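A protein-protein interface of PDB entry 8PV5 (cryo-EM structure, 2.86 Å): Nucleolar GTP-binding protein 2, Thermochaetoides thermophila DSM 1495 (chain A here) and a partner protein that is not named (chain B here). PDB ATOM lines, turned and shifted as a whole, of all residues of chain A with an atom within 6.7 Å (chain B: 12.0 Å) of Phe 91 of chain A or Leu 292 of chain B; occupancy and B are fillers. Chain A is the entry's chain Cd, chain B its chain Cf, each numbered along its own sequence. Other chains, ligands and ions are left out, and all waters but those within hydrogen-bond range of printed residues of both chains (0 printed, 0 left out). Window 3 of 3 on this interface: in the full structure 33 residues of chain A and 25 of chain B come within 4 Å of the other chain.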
ATOM      1  N   ILE A  83      22.664 -31.669 -27.722  1.00  0.00           N
ATOM      2  CA  ILE A  83      21.341 -31.065 -27.812  1.00  0.00           C
ATOM      3  C   ILE A  83      20.931 -31.031 -29.279  1.00  0.00           C
ATOM      4  O   ILE A  83      21.778 -30.909 -30.170  1.00  0.00           O
ATOM      5  CB  ILE A  83      21.320 -29.663 -27.156  1.00  0.00           C
ATOM      6  CG1 ILE A  83      19.892 -29.130 -27.019  1.00  0.00           C
ATOM      7  CG2 ILE A  83      22.219 -28.681 -27.899  1.00  0.00           C
ATOM      8  CD1 ILE A  83      19.771 -27.953 -26.086  1.00  0.00           C
ATOM      9  N   ASP A  86      15.774 -29.135 -32.819  1.00  0.00           N
ATOM     10  CA  ASP A  86      14.381 -28.939 -32.431  1.00  0.00           C
ATOM     11  C   ASP A  86      14.278 -28.478 -30.983  1.00  0.00           C
ATOM     12  O   ASP A  86      13.482 -27.591 -30.652  1.00  0.00           O
ATOM     13  CB  ASP A  86      13.597 -30.233 -32.639  1.00  0.00           C
ATOM     14  CG  ASP A  86      13.432 -30.586 -34.101  1.00  0.00           C
ATOM     15  OD1 ASP A  86      13.399 -29.660 -34.938  1.00  0.00           O
ATOM     16  OD2 ASP A  86      13.333 -31.791 -34.414  1.00  0.00           O
ATOM     17  N   THR A  87      15.089 -29.074 -30.105  1.00  0.00           N
ATOM     18  CA  THR A  87      15.111 -28.671 -28.704  1.00  0.00           C
ATOM     19  C   THR A  87      15.624 -27.244 -28.550  1.00  0.00           C
ATOM     20  O   THR A  87      15.087 -26.465 -27.750  1.00  0.00           O
ATOM     21  CB  THR A  87      15.971 -29.651 -27.905  1.00  0.00           C
ATOM     22  OG1 THR A  87      15.474 -30.981 -28.098  1.00  0.00           O
ATOM     23  CG2 THR A  87      15.925 -29.328 -26.426  1.00  0.00           C
ATOM     24  N   LEU A  88      16.654 -26.880 -29.322  1.00  0.00           N
ATOM     25  CA  LEU A  88      17.164 -25.511 -29.287  1.00  0.00           C
ATOM     26  C   LEU A  88      16.116 -24.513 -29.768  1.00  0.00           C
ATOM     27  O   LEU A  88      15.960 -23.439 -29.177  1.00  0.00           O
ATOM     28  CB  LEU A  88      18.434 -25.403 -30.129  1.00  0.00           C
ATOM     29  CG  LEU A  88      19.732 -25.857 -29.459  1.00  0.00           C
ATOM     30  CD1 LEU A  88      20.860 -25.955 -30.474  1.00  0.00           C
ATOM     31  CD2 LEU A  88      20.106 -24.913 -28.331  1.00  0.00           C
ATOM     32  N   GLN A  89      15.380 -24.857 -30.829  1.00  0.00           N
ATOM     33  CA  GLN A  89      14.322 -23.979 -31.324  1.00  0.00           C
ATOM     34  C   GLN A  89      13.197 -23.833 -30.305  1.00  0.00           C
ATOM     35  O   GLN A  89      12.649 -22.736 -30.126  1.00  0.00           O
ATOM     36  CB  GLN A  89      13.779 -24.510 -32.650  1.00  0.00           C
ATOM     37  CG  GLN A  89      12.930 -23.516 -33.424  1.00  0.00           C
ATOM     38  CD  GLN A  89      13.606 -22.170 -33.586  1.00  0.00           C
ATOM     39  OE1 GLN A  89      13.108 -21.150 -33.110  1.00  0.00           O
ATOM     40  NE2 GLN A  89      14.751 -22.161 -34.255  1.00  0.00           N
ATOM     41  N   SER A  90      12.844 -24.929 -29.625  1.00  0.00           N
ATOM     42  CA  SER A  90      11.827 -24.872 -28.579  1.00  0.00           C
ATOM     43  C   SER A  90      12.274 -23.979 -27.427  1.00  0.00           C
ATOM     44  O   SER A  90      11.481 -23.201 -26.886  1.00  0.00           O
ATOM     45  CB  SER A  90      11.517 -26.281 -28.077  1.00  0.00           C
ATOM     46  OG  SER A  90      11.109 -27.124 -29.140  1.00  0.00           O
ATOM     47  N   PHE A  91      13.552 -24.071 -27.050  1.00  0.00           N
ATOM     48  CA  PHE A  91      14.067 -23.226 -25.976  1.00  0.00           C
ATOM     49  C   PHE A  91      14.107 -21.758 -26.386  1.00  0.00           C
ATOM     50  O   PHE A  91      13.848 -20.870 -25.563  1.00  0.00           O
ATOM     51  CB  PHE A  91      15.454 -23.703 -25.552  1.00  0.00           C
ATOM     52  CG  PHE A  91      15.428 -24.881 -24.627  1.00  0.00           C
ATOM     53  CD1 PHE A  91      14.420 -25.018 -23.689  1.00  0.00           C
ATOM     54  CD2 PHE A  91      16.414 -25.850 -24.689  1.00  0.00           C
ATOM     55  CE1 PHE A  91      14.393 -26.099 -22.831  1.00  0.00           C
ATOM     56  CE2 PHE A  91      16.391 -26.933 -23.833  1.00  0.00           C
ATOM     57  CZ  PHE A  91      15.378 -27.058 -22.905  1.00  0.00           C
ATOM     58  N   ARG A  92      14.431 -21.483 -27.653  1.00  0.00           N
ATOM     59  CA  ARG A  92      14.411 -20.107 -28.144  1.00  0.00           C
ATOM     60  C   ARG A  92      13.002 -19.532 -28.124  1.00  0.00           C
ATOM     61  O   ARG A  92      12.798 -18.381 -27.716  1.00  0.00           O
ATOM     62  CB  ARG A  92      14.979 -20.042 -29.560  1.00  0.00           C
ATOM     63  CG  ARG A  92      16.460 -20.325 -29.660  1.00  0.00           C
ATOM     64  CD  ARG A  92      16.980 -20.018 -31.048  1.00  0.00           C
ATOM     65  NE  ARG A  92      18.307 -20.583 -31.257  1.00  0.00           N
ATOM     66  CZ  ARG A  92      18.546 -21.684 -31.956  1.00  0.00           C
ATOM     67  NH1 ARG A  92      17.570 -22.354 -32.545  1.00  0.00           N
ATOM     68  NH2 ARG A  92      19.797 -22.119 -32.073  1.00  0.00           N
ATOM     69  N   GLU A  93      12.016 -20.324 -28.558  1.00  0.00           N
ATOM     70  CA  GLU A  93      10.625 -19.881 -28.496  1.00  0.00           C
ATOM     71  C   GLU A  93      10.181 -19.660 -27.057  1.00  0.00           C
ATOM     72  O   GLU A  93       9.457 -18.701 -26.761  1.00  0.00           O
ATOM     73  CB  GLU A  93       9.715 -20.895 -29.187  1.00  0.00           C
ATOM     74  CG  GLU A  93       9.916 -20.985 -30.690  1.00  0.00           C
ATOM     75  CD  GLU A  93       9.400 -22.289 -31.265  1.00  0.00           C
ATOM     76  OE1 GLU A  93       9.051 -23.187 -30.472  1.00  0.00           O
ATOM     77  OE2 GLU A  93       9.341 -22.416 -32.507  1.00  0.00           O
ATOM     78  N   ALA A  94      10.618 -20.531 -26.145  1.00  0.00           N
ATOM     79  CA  ALA A  94      10.276 -20.382 -24.735  1.00  0.00           C
ATOM     80  C   ALA A  94      10.850 -19.099 -24.150  1.00  0.00           C
ATOM     81  O   ALA A  94      10.159 -18.372 -23.425  1.00  0.00           O
ATOM     82  CB  ALA A  94      10.783 -21.588 -23.953  1.00  0.00           C
ATOM     83  N   MET A  95      12.113 -18.802 -24.461  1.00  0.00           N
ATOM     84  CA  MET A  95      12.747 -17.606 -23.916  1.00  0.00           C
ATOM     85  C   MET A  95      12.170 -16.343 -24.545  1.00  0.00           C
ATOM     86  O   MET A  95      12.122 -15.284 -23.908  1.00  0.00           O
ATOM     87  CB  MET A  95      14.261 -17.681 -24.102  1.00  0.00           C
ATOM     88  CG  MET A  95      15.013 -16.534 -23.455  1.00  0.00           C
ATOM     89  SD  MET A  95      16.793 -16.666 -23.683  1.00  0.00           S
ATOM     90  CE  MET A  95      17.177 -18.030 -22.584  1.00  0.00           C
ATOM     91  N   ALA A  96      11.719 -16.436 -25.799  1.00  0.00           N
ATOM     92  CA  ALA A  96      10.990 -15.324 -26.402  1.00  0.00           C
ATOM     93  C   ALA A  96       9.638 -15.124 -25.725  1.00  0.00           C
ATOM     94  O   ALA A  96       9.171 -13.989 -25.575  1.00  0.00           O
ATOM     95  CB  ALA A  96      10.814 -15.569 -27.898  1.00  0.00           C
ATOM     96  N   LYS A  98       9.011 -15.791 -22.578  1.00  0.00           N
ATOM     97  CA  LYS A  98       9.202 -15.561 -21.144  1.00  0.00           C
ATOM     98  C   LYS A  98       8.671 -14.211 -20.669  1.00  0.00           C
ATOM     99  O   LYS A  98       8.833 -13.187 -21.340  1.00  0.00           O
ATOM    100  CB  LYS A  98      10.686 -15.653 -20.793  1.00  0.00           C
ATOM    101  CG  LYS A  98      11.209 -17.048 -20.554  1.00  0.00           C
ATOM    102  CD  LYS A  98      12.690 -16.987 -20.231  1.00  0.00           C
ATOM    103  CE  LYS A  98      12.941 -16.340 -18.880  1.00  0.00           C
ATOM    104  NZ  LYS A  98      14.386 -16.357 -18.522  1.00  0.00           N
ATOM    105  N   ASN A 110      18.499 -24.699 -14.809  1.00  0.00           N
ATOM    106  CA  ASN A 110      18.691 -25.783 -15.762  1.00  0.00           C
ATOM    107  C   ASN A 110      19.971 -25.530 -16.548  1.00  0.00           C
ATOM    108  O   ASN A 110      20.163 -24.439 -17.096  1.00  0.00           O
ATOM    109  CB  ASN A 110      17.492 -25.895 -16.701  1.00  0.00           C
ATOM    110  CG  ASN A 110      17.528 -27.149 -17.547  1.00  0.00           C
ATOM    111  OD1 ASN A 110      18.296 -28.070 -17.280  1.00  0.00           O
ATOM    112  ND2 ASN A 110      16.695 -27.188 -18.579  1.00  0.00           N
ATOM    113  N   LYS A 111      20.848 -26.531 -16.593  1.00  0.00           N
ATOM    114  CA  LYS A 111      22.100 -26.415 -17.332  1.00  0.00           C
ATOM    115  C   LYS A 111      21.808 -26.477 -18.825  1.00  0.00           C
ATOM    116  O   LYS A 111      21.509 -27.547 -19.364  1.00  0.00           O
ATOM    117  CB  LYS A 111      23.067 -27.517 -16.914  1.00  0.00           C
ATOM    118  CG  LYS A 111      23.396 -27.515 -15.435  1.00  0.00           C
ATOM    119  CD  LYS A 111      24.324 -28.659 -15.073  1.00  0.00           C
ATOM    120  CE  LYS A 111      24.732 -28.590 -13.613  1.00  0.00           C
ATOM    121  NZ  LYS A 111      23.559 -28.656 -12.702  1.00  0.00           N
ATOM    122  N   LEU A 112      21.892 -25.336 -19.492  1.00  0.00           N
ATOM    123  CA  LEU A 112      21.540 -25.212 -20.896  1.00  0.00           C
ATOM    124  C   LEU A 112      22.640 -24.450 -21.617  1.00  0.00           C
ATOM    125  O   LEU A 112      23.333 -23.628 -21.010  1.00  0.00           O
ATOM    126  CB  LEU A 112      20.199 -24.486 -21.067  1.00  0.00           C
ATOM    127  CG  LEU A 112      18.959 -25.276 -20.661  1.00  0.00           C
ATOM    128  CD1 LEU A 112      17.697 -24.477 -20.939  1.00  0.00           C
ATOM    129  CD2 LEU A 112      18.935 -26.619 -21.367  1.00  0.00           C
ATOM    130  N   PRO A 113      22.831 -24.708 -22.922  1.00  0.00           N
ATOM    131  CA  PRO A 113      23.770 -23.876 -23.708  1.00  0.00           C
ATOM    132  C   PRO A 113      23.165 -22.506 -23.998  1.00  0.00           C
ATOM    133  O   PRO A 113      22.531 -22.261 -25.021  1.00  0.00           O
ATOM    134  CB  PRO A 113      23.980 -24.710 -24.974  1.00  0.00           C
ATOM    135  CG  PRO A 113      22.726 -25.505 -25.121  1.00  0.00           C
ATOM    136  CD  PRO A 113      22.222 -25.779 -23.734  1.00  0.00           C
ATOM    137  N   MET A 114      23.368 -21.586 -23.051  1.00  0.00           N
ATOM    138  CA  MET A 114      22.654 -20.311 -23.063  1.00  0.00           C
ATOM    139  C   MET A 114      23.083 -19.424 -24.223  1.00  0.00           C
ATOM    140  O   MET A 114      22.287 -18.609 -24.707  1.00  0.00           O
ATOM    141  CB  MET A 114      22.887 -19.589 -21.740  1.00  0.00           C
ATOM    142  CG  MET A 114      22.097 -20.158 -20.579  1.00  0.00           C
ATOM    143  SD  MET A 114      20.372 -19.658 -20.589  1.00  0.00           S
ATOM    144  CE  MET A 114      20.547 -17.933 -21.026  1.00  0.00           C
ATOM    145  N   ILE A 117      20.936 -20.116 -27.186  1.00  0.00           N
ATOM    146  CA  ILE A 117      19.509 -19.937 -26.955  1.00  0.00           C
ATOM    147  C   ILE A 117      19.125 -18.467 -26.857  1.00  0.00           C
ATOM    148  O   ILE A 117      18.125 -18.044 -27.453  1.00  0.00           O
ATOM    149  CB  ILE A 117      19.043 -20.709 -25.697  1.00  0.00           C
ATOM    150  CG1 ILE A 117      19.353 -22.198 -25.845  1.00  0.00           C
ATOM    151  CG2 ILE A 117      17.555 -20.511 -25.449  1.00  0.00           C
ATOM    152  CD1 ILE A 117      19.063 -23.011 -24.605  1.00  0.00           C
ATOM    153  N   SER B 288       6.957 -26.043  -9.542  1.00  0.00           N
ATOM    154  CA  SER B 288       6.663 -26.304 -10.942  1.00  0.00           C
ATOM    155  C   SER B 288       7.962 -26.248 -11.730  1.00  0.00           C
ATOM    156  O   SER B 288       9.033 -25.977 -11.188  1.00  0.00           O
ATOM    157  CB  SER B 288       5.640 -25.308 -11.497  1.00  0.00           C
ATOM    158  OG  SER B 288       6.182 -24.003 -11.571  1.00  0.00           O
ATOM    159  N   MET B 289       7.854 -26.519 -13.024  1.00  0.00           N
ATOM    160  CA  MET B 289       8.968 -26.407 -13.953  1.00  0.00           C
ATOM    161  C   MET B 289       8.548 -25.499 -15.097  1.00  0.00           C
ATOM    162  O   MET B 289       7.487 -25.703 -15.695  1.00  0.00           O
ATOM    163  CB  MET B 289       9.380 -27.780 -14.483  1.00  0.00           C
ATOM    164  CG  MET B 289      10.570 -27.754 -15.416  1.00  0.00           C
ATOM    165  SD  MET B 289      11.029 -29.397 -15.990  1.00  0.00           S
ATOM    166  CE  MET B 289       9.679 -29.753 -17.111  1.00  0.00           C
ATOM    167  N   ASP B 290       9.375 -24.502 -15.406  1.00  0.00           N
ATOM    168  CA  ASP B 290       8.984 -23.554 -16.439  1.00  0.00           C
ATOM    169  C   ASP B 290       9.275 -24.126 -17.826  1.00  0.00           C
ATOM    170  O   ASP B 290       9.580 -25.310 -17.993  1.00  0.00           O
ATOM    171  CB  ASP B 290       9.664 -22.201 -16.218  1.00  0.00           C
ATOM    172  CG  ASP B 290      11.172 -22.249 -16.392  1.00  0.00           C
ATOM    173  OD1 ASP B 290      11.758 -23.349 -16.417  1.00  0.00           O
ATOM    174  OD2 ASP B 290      11.780 -21.164 -16.509  1.00  0.00           O
ATOM    175  N   LEU B 291       9.183 -23.269 -18.842  1.00  0.00           N
ATOM    176  CA  LEU B 291       9.397 -23.723 -20.209  1.00  0.00           C
ATOM    177  C   LEU B 291      10.872 -23.919 -20.538  1.00  0.00           C
ATOM    178  O   LEU B 291      11.185 -24.572 -21.539  1.00  0.00           O
ATOM    179  CB  LEU B 291       8.762 -22.738 -21.187  1.00  0.00           C
ATOM    180  CG  LEU B 291       7.236 -22.748 -21.276  1.00  0.00           C
ATOM    181  CD1 LEU B 291       6.753 -21.705 -22.272  1.00  0.00           C
ATOM    182  CD2 LEU B 291       6.735 -24.131 -21.657  1.00  0.00           C
ATOM    183  N   LEU B 292      11.781 -23.374 -19.732  1.00  0.00           N
ATOM    184  CA  LEU B 292      13.212 -23.579 -19.915  1.00  0.00           C
ATOM    185  C   LEU B 292      13.770 -24.684 -19.027  1.00  0.00           C
ATOM    186  O   LEU B 292      14.983 -24.913 -19.033  1.00  0.00           O
ATOM    187  CB  LEU B 292      13.981 -22.284 -19.656  1.00  0.00           C
ATOM    188  CG  LEU B 292      14.045 -21.259 -20.785  1.00  0.00           C
ATOM    189  CD1 LEU B 292      14.728 -20.006 -20.286  1.00  0.00           C
ATOM    190  CD2 LEU B 292      14.780 -21.825 -21.982  1.00  0.00           C
ATOM    191  N   GLY B 293      12.925 -25.366 -18.264  1.00  0.00           N
ATOM    192  CA  GLY B 293      13.384 -26.425 -17.395  1.00  0.00           C
ATOM    193  C   GLY B 293      13.814 -25.994 -16.011  1.00  0.00           C
ATOM    194  O   GLY B 293      14.196 -26.853 -15.207  1.00  0.00           O
ATOM    195  N   ASP B 294      13.779 -24.700 -15.711  1.00  0.00           N
ATOM    196  CA  ASP B 294      14.091 -24.224 -14.373  1.00  0.00           C
ATOM    197  C   ASP B 294      12.984 -24.607 -13.401  1.00  0.00           C
ATOM    198  O   ASP B 294      11.790 -24.527 -13.715  1.00  0.00           O
ATOM    199  CB  ASP B 294      14.271 -22.705 -14.367  1.00  0.00           C
ATOM    200  CG  ASP B 294      15.460 -22.252 -15.188  1.00  0.00           C
ATOM    201  OD1 ASP B 294      16.342 -23.086 -15.473  1.00  0.00           O
ATOM    202  OD2 ASP B 294      15.512 -21.058 -15.546  1.00  0.00           O
ATOM    203  N   LYS B 295      13.393 -25.028 -12.206  1.00  0.00           N
ATOM    204  CA  LYS B 295      12.450 -25.313 -11.136  1.00  0.00           C
ATOM    205  C   LYS B 295      12.025 -24.007 -10.477  1.00  0.00           C
ATOM    206  O   LYS B 295      12.867 -23.205 -10.066  1.00  0.00           O
ATOM    207  CB  LYS B 295      13.071 -26.253 -10.106  1.00  0.00           C
ATOM    208  CG  LYS B 295      12.099 -26.745  -9.049  1.00  0.00           C
ATOM    209  CD  LYS B 295      12.811 -27.562  -7.988  1.00  0.00           C
ATOM    210  CE  LYS B 295      13.471 -28.787  -8.590  1.00  0.00           C
ATOM    211  NZ  LYS B 295      14.244 -29.552  -7.578  1.00  0.00           N
ATOM    212  N   ILE B 296      10.716 -23.801 -10.378  1.00  0.00           N
ATOM    213  CA  ILE B 296      10.131 -22.541  -9.944  1.00  0.00           C
ATOM    214  C   ILE B 296       9.300 -22.789  -8.694  1.00  0.00           C
ATOM    215  O   ILE B 296       8.492 -23.724  -8.649  1.00  0.00           O
ATOM    216  CB  ILE B 296       9.271 -21.911 -11.059  1.00  0.00           C
ATOM    217  CG1 ILE B 296      10.085 -21.761 -12.343  1.00  0.00           C
ATOM    218  CG2 ILE B 296       8.726 -20.567 -10.629  1.00  0.00           C
ATOM    219  CD1 ILE B 296      11.309 -20.888 -12.184  1.00  0.00           C
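N of Asn 110 of chain A lies within hydrogen-bond range of OD1 of Asp 294 of chain B (2.8 Å).
The side-chain amide nitrogen (ND2) of Asn 110 of chain A is in hydrogen-bond range of the backbone carbonyl oxygen (O) of Leu 292 of chain B, at 2.9 Å.
OD1 of Asp 290 of chain B sits close to N of Leu 292 of chain B.
The backbone NH (N) of Gly 293 of chain B is in hydrogen-bond range of the side-chain carboxylate (OD1) of Asp 290 of chain B, at 3.0 Å.
OD1 of Asp 290 of chain B sits at hydrogen-bond distance from N of Asp 294 of chain B, at 2.5 Å.
Among the printed residues, merely in contact across the chains: Leu 112 of chain A with Leu 292 of chain B, Asn 110 of chain A with Gly 293 of chain B, Ala 94 of chain A with Leu 291 of chain B, Phe 91 of chain A with Leu 292 of chain B, Lys 98 of chain A with Leu 292 of chain B, Phe 91 of chain A with Leu 291 of chain B and Met 95 of chain A with Leu 292 of chain B.
Leu 292 of chain B touches five residues of chain A.
No residue of chain B comes within 4 Å of Thr 87 of chain A.
No residue of chain B comes within 4 Å of Leu 88 of chain A.
No residue of chain B comes within 4 Å of Gln 89 of chain A.
No residue of chain B comes within 4 Å of Ser 90 of chain A.
Glu 93 of chain A touches none of the printed residues of chain B.
No residue of chain B comes within 4 Å of Pro 113 of chain A.
No residue of chain B comes within 4 Å of Ile 117 of chain A.
Of the printed residues of chain A, Asp 294 of chain B touches Asn 110 (2.8 Å).
Printed residues of chain A within 4 Å of Gly 293 of chain B: Asn 110 (3.6 Å).
The nearest residue of chain B that does not touch Phe 91 of chain A is Gly 293 of chain B (4.9 Å).
Of the 9 printed residues of chain B, 4 touch a printed residue of chain A.
Printed residues of chain B that touch a printed residue of chain A: Leu 291, Leu 292, Gly 293 and Asp 294.
Hydrophobic or aromatic side chains of chain B within 4 Å of the printed part of chain A: Leu 291 and Leu 292.
Of the 19 printed residues of chain A, 6 touch a printed residue of chain B.
Printed residues of chain A that touch a printed residue of chain B: Phe 91, Ala 94, Met 95, Lys 98, Asn 110 and Leu 112.
Hydrophobic or aromatic side chains of chain A within 4 Å of the printed part of chain B: Phe 91, Ala 94, Met 95 and Leu 112.
Among the printed residues, 9 pairs touch across the chains.
Among the printed residues, no Asp or Glu carboxylate lies within 4 Å of a Lys or Arg side-chain nitrogen of the other chain.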
